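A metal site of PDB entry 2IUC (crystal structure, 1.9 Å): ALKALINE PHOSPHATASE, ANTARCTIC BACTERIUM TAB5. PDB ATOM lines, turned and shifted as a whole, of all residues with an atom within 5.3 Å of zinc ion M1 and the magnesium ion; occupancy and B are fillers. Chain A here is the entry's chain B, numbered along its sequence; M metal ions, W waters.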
ATOM      1  N   ASP A  43       5.711 -24.168  -7.463  1.00  0.00           N
ATOM      2  CA  ASP A  43       5.071 -23.953  -8.746  1.00  0.00           C
ATOM      3  C   ASP A  43       5.923 -23.023  -9.609  1.00  0.00           C
ATOM      4  O   ASP A  43       6.276 -21.974  -9.151  1.00  0.00           O
ATOM      5  CB  ASP A  43       3.707 -23.293  -8.491  1.00  0.00           C
ATOM      6  CG  ASP A  43       2.720 -23.413  -9.699  1.00  0.00           C
ATOM      7  OD1 ASP A  43       3.043 -22.907 -10.791  1.00  0.00           O
ATOM      8  OD2 ASP A  43       1.594 -23.896  -9.514  1.00  0.00           O
ATOM      9  N   GLY A  44       6.239 -23.367 -10.863  1.00  0.00           N
ATOM     10  CA  GLY A  44       6.913 -22.353 -11.681  1.00  0.00           C
ATOM     11  C   GLY A  44       8.425 -22.406 -11.498  1.00  0.00           C
ATOM     12  O   GLY A  44       9.117 -21.603 -12.079  1.00  0.00           O
ATOM     13  N   ASP A  83       0.065 -26.137 -18.131  1.00  0.00           N
ATOM     14  CA  ASP A  83      -0.334 -25.224 -17.000  1.00  0.00           C
ATOM     15  C   ASP A  83      -0.268 -25.950 -15.652  1.00  0.00           C
ATOM     16  O   ASP A  83       0.012 -27.171 -15.594  1.00  0.00           O
ATOM     17  CB  ASP A  83      -1.673 -24.538 -17.278  1.00  0.00           C
ATOM     18  CG  ASP A  83      -2.934 -25.421 -16.912  1.00  0.00           C
ATOM     19  OD1 ASP A  83      -2.900 -26.679 -16.904  1.00  0.00           O
ATOM     20  OD2 ASP A  83      -3.995 -24.825 -16.627  1.00  0.00           O
ATOM     21  N   SER A  84      -0.565 -25.246 -14.572  1.00  0.00           N
ATOM     22  CA  SER A  84      -0.554 -25.831 -13.226  1.00  0.00           C
ATOM     23  C   SER A  84      -1.565 -26.938 -13.002  1.00  0.00           C
ATOM     24  O   SER A  84      -1.336 -27.855 -12.214  1.00  0.00           O
ATOM     25  CB  SER A  84      -0.843 -24.749 -12.232  1.00  0.00           C
ATOM     26  OG  SER A  84       0.091 -23.693 -12.457  1.00  0.00           O
ATOM     27  N   SER A 131      -1.212 -19.747  -2.117  1.00  0.00           N
ATOM     28  CA  SER A 131      -2.314 -19.198  -2.905  1.00  0.00           C
ATOM     29  C   SER A 131      -3.647 -19.427  -2.176  1.00  0.00           C
ATOM     30  O   SER A 131      -3.678 -19.960  -1.046  1.00  0.00           O
ATOM     31  CB  SER A 131      -2.378 -19.931  -4.283  1.00  0.00           C
ATOM     32  OG  SER A 131      -2.618 -21.341  -4.098  1.00  0.00           O
ATOM     33  N   HIS A 135      -6.975 -22.758  -5.733  1.00  0.00           N
ATOM     34  CA  HIS A 135      -6.089 -22.488  -6.890  1.00  0.00           C
ATOM     35  C   HIS A 135      -5.583 -23.807  -7.465  1.00  0.00           C
ATOM     36  O   HIS A 135      -5.749 -24.840  -6.841  1.00  0.00           O
ATOM     37  CB  HIS A 135      -4.987 -21.529  -6.487  1.00  0.00           C
ATOM     38  CG  HIS A 135      -4.373 -20.819  -7.648  1.00  0.00           C
ATOM     39  ND1 HIS A 135      -3.253 -21.295  -8.290  1.00  0.00           N
ATOM     40  CD2 HIS A 135      -4.664 -19.623  -8.228  1.00  0.00           C
ATOM     41  CE1 HIS A 135      -2.906 -20.445  -9.243  1.00  0.00           C
ATOM     42  NE2 HIS A 135      -3.767 -19.433  -9.258  1.00  0.00           N
ATOM     43  N   ALA A 136      -5.086 -23.839  -8.722  1.00  0.00           N
ATOM     44  CA  ALA A 136      -5.112 -25.130  -9.457  1.00  0.00           C
ATOM     45  C   ALA A 136      -4.325 -26.285  -8.815  1.00  0.00           C
ATOM     46  O   ALA A 136      -4.691 -27.479  -8.932  1.00  0.00           O
ATOM     47  CB  ALA A 136      -4.641 -24.950 -10.981  1.00  0.00           C
ATOM     48  N   THR A 137      -3.167 -25.965  -8.194  1.00  0.00           N
ATOM     49  CA  THR A 137      -2.280 -27.007  -7.624  1.00  0.00           C
ATOM     50  C   THR A 137      -2.935 -27.704  -6.426  1.00  0.00           C
ATOM     51  O   THR A 137      -3.185 -28.959  -6.503  1.00  0.00           O
ATOM     52  CB  THR A 137      -0.874 -26.429  -7.290  1.00  0.00           C
ATOM     53  OG1 THR A 137      -0.381 -25.692  -8.399  1.00  0.00           O
ATOM     54  CG2 THR A 137       0.169 -27.544  -6.867  1.00  0.00           C
ATOM     55  N   PRO A 138      -3.302 -26.918  -5.355  1.00  0.00           N
ATOM     56  CA  PRO A 138      -4.032 -27.565  -4.214  1.00  0.00           C
ATOM     57  C   PRO A 138      -5.363 -28.246  -4.709  1.00  0.00           C
ATOM     58  O   PRO A 138      -5.651 -29.359  -4.286  1.00  0.00           O
ATOM     59  CB  PRO A 138      -4.264 -26.426  -3.221  1.00  0.00           C
ATOM     60  CG  PRO A 138      -4.035 -25.098  -4.013  1.00  0.00           C
ATOM     61  CD  PRO A 138      -3.125 -25.449  -5.166  1.00  0.00           C
ATOM     62  N   GLU A 254       2.492 -26.502  -1.077  1.00  0.00           N
ATOM     63  CA  GLU A 254       2.846 -25.804  -2.291  1.00  0.00           C
ATOM     64  C   GLU A 254       3.422 -24.442  -1.983  1.00  0.00           C
ATOM     65  O   GLU A 254       2.822 -23.668  -1.205  1.00  0.00           O
ATOM     66  CB  GLU A 254       1.627 -25.622  -3.170  1.00  0.00           C
ATOM     67  CG  GLU A 254       2.041 -25.128  -4.557  1.00  0.00           C
ATOM     68  CD  GLU A 254       0.967 -24.410  -5.366  1.00  0.00           C
ATOM     69  OE1 GLU A 254      -0.069 -24.024  -4.794  1.00  0.00           O
ATOM     70  OE2 GLU A 254       1.176 -24.161  -6.596  1.00  0.00           O
ATOM     71  N   SER A 256       3.331 -21.611  -3.799  1.00  0.00           N
ATOM     72  CA  SER A 256       2.464 -21.227  -4.874  1.00  0.00           C
ATOM     73  C   SER A 256       2.892 -20.006  -5.659  1.00  0.00           C
ATOM     74  O   SER A 256       2.583 -19.891  -6.867  1.00  0.00           O
ATOM     75  CB  SER A 256       1.042 -20.962  -4.324  1.00  0.00           C
ATOM     76  OG  SER A 256       0.653 -21.965  -3.372  1.00  0.00           O
ATOM     77  N   ASP A 259       5.768 -19.054  -8.997  1.00  0.00           N
ATOM     78  CA  ASP A 259       5.167 -18.862 -10.326  1.00  0.00           C
ATOM     79  C   ASP A 259       4.756 -17.432 -10.647  1.00  0.00           C
ATOM     80  O   ASP A 259       4.936 -16.918 -11.747  1.00  0.00           O
ATOM     81  CB  ASP A 259       3.919 -19.742 -10.411  1.00  0.00           C
ATOM     82  CG  ASP A 259       3.206 -19.698 -11.776  1.00  0.00           C
ATOM     83  OD1 ASP A 259       3.766 -20.107 -12.763  1.00  0.00           O
ATOM     84  OD2 ASP A 259       2.043 -19.301 -11.854  1.00  0.00           O
ATOM     85  N   ASP A 301       5.845 -28.159 -11.086  1.00  0.00           N
ATOM     86  CA  ASP A 301       4.930 -28.569 -12.109  1.00  0.00           C
ATOM     87  C   ASP A 301       5.452 -28.180 -13.524  1.00  0.00           C
ATOM     88  O   ASP A 301       5.117 -28.845 -14.499  1.00  0.00           O
ATOM     89  CB  ASP A 301       3.506 -28.006 -11.821  1.00  0.00           C
ATOM     90  CG  ASP A 301       3.481 -26.480 -11.636  1.00  0.00           C
ATOM     91  OD1 ASP A 301       4.586 -25.883 -11.379  1.00  0.00           O
ATOM     92  OD2 ASP A 301       2.346 -25.886 -11.786  1.00  0.00           O
ATOM     93  N   HIS A 302       6.232 -27.113 -13.587  1.00  0.00           N
ATOM     94  CA  HIS A 302       6.778 -26.524 -14.853  1.00  0.00           C
ATOM     95  C   HIS A 302       7.656 -25.342 -14.377  1.00  0.00           C
ATOM     96  O   HIS A 302       7.673 -24.969 -13.157  1.00  0.00           O
ATOM     97  CB  HIS A 302       5.638 -26.003 -15.792  1.00  0.00           C
ATOM     98  CG  HIS A 302       4.776 -24.963 -15.116  1.00  0.00           C
ATOM     99  ND1 HIS A 302       5.178 -23.633 -14.966  1.00  0.00           N
ATOM    100  CD2 HIS A 302       3.611 -25.086 -14.425  1.00  0.00           C
ATOM    101  CE1 HIS A 302       4.282 -22.996 -14.213  1.00  0.00           C
ATOM    102  NE2 HIS A 302       3.314 -23.850 -13.904  1.00  0.00           N
ATOM    103  N   HIS A 337       4.805 -19.913 -19.126  1.00  0.00           N
ATOM    104  CA  HIS A 337       5.493 -21.104 -18.697  1.00  0.00           C
ATOM    105  C   HIS A 337       6.476 -21.556 -19.799  1.00  0.00           C
ATOM    106  O   HIS A 337       6.378 -21.123 -20.958  1.00  0.00           O
ATOM    107  CB  HIS A 337       4.501 -22.275 -18.397  1.00  0.00           C
ATOM    108  CG  HIS A 337       3.488 -21.942 -17.338  1.00  0.00           C
ATOM    109  ND1 HIS A 337       2.393 -22.743 -17.089  1.00  0.00           N
ATOM    110  CD2 HIS A 337       3.376 -20.867 -16.525  1.00  0.00           C
ATOM    111  CE1 HIS A 337       1.650 -22.179 -16.133  1.00  0.00           C
ATOM    112  NE2 HIS A 337       2.248 -21.059 -15.768  1.00  0.00           N
HETATM  113 ZN    ZN M   1       2.172 -23.864 -12.246  1.00  0.00          ZN
HETATM  114 MG    MG M   2       0.064 -23.506  -7.984  1.00  0.00          MG
HETATM  115 ZN    ZN M   3       1.839 -19.865 -14.115  1.00  0.00          ZN
HETATM  116  O   HOH W   1      -1.414 -23.101  -9.755  1.00  0.00           O
HETATM  117  O   HOH W   2      -1.749 -23.006  -6.879  1.00  0.00           O
HETATM  118  O   HOH W   3       0.645 -21.437  -8.056  1.00  0.00           O
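The magnesium ion is bound by the side-chain carboxylate of Glu 254 (1.9 Å), water W3 (2.2 Å), water W2 (2.2 Å), the side-chain carboxylate of Asp 43 (2.2 Å), the side-chain hydroxyl of Thr 137 (2.3 Å) and water W1 (2.3 Å). The magnesium ion has six donor atoms within binding distance.
The backbone carbonyl oxygen (O) of His 302 sits close to the backbone NH (N) of Gly 44, 3.1 Å away. A ring nitrogen (NE2) of His 302 lies close to a ring nitrogen (ND1) of His 337, at 3.5 Å. The side-chain carboxylate (OE1) of Glu 254 sits at hydrogen-bond distance from the side-chain hydroxyl (OG) of Ser 256, 2.6 Å away. N of Gly 44 is in hydrogen-bond range of OD1 of Asp 301 (3.1 Å). O of Asp 43 sits at hydrogen-bond distance from N of Asp 259 (3.0 Å).
Water W2 lies within hydrogen-bond range of ND1 of His 135 (2.7 Å), OE1 of Glu 254 (2.9 Å) and OG of Ser 131 (3.4 Å).
His 135 touches the magnesium ion (ND1 to MG, 3.998 Å). Along chain A the residues within 4 Å of the magnesium ion span positions 43 to 254. The nearest printed residue that does not touch the magnesium ion is Ser 84 (4.5 Å).
Zinc ion M1 is bound by the side-chain carboxylate of Asp 43, a ring nitrogen (NE2) of His 302, the side-chain carboxylate of Asp 301 and the side-chain hydroxyl of Ser 84. Slightly farther from zinc ion M1 lies the side-chain carboxylate (OD2) of Asp 43 (2.8 Å).
The nearest printed residue that does not touch zinc ion M1 is Asp 259 (4.1 Å).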
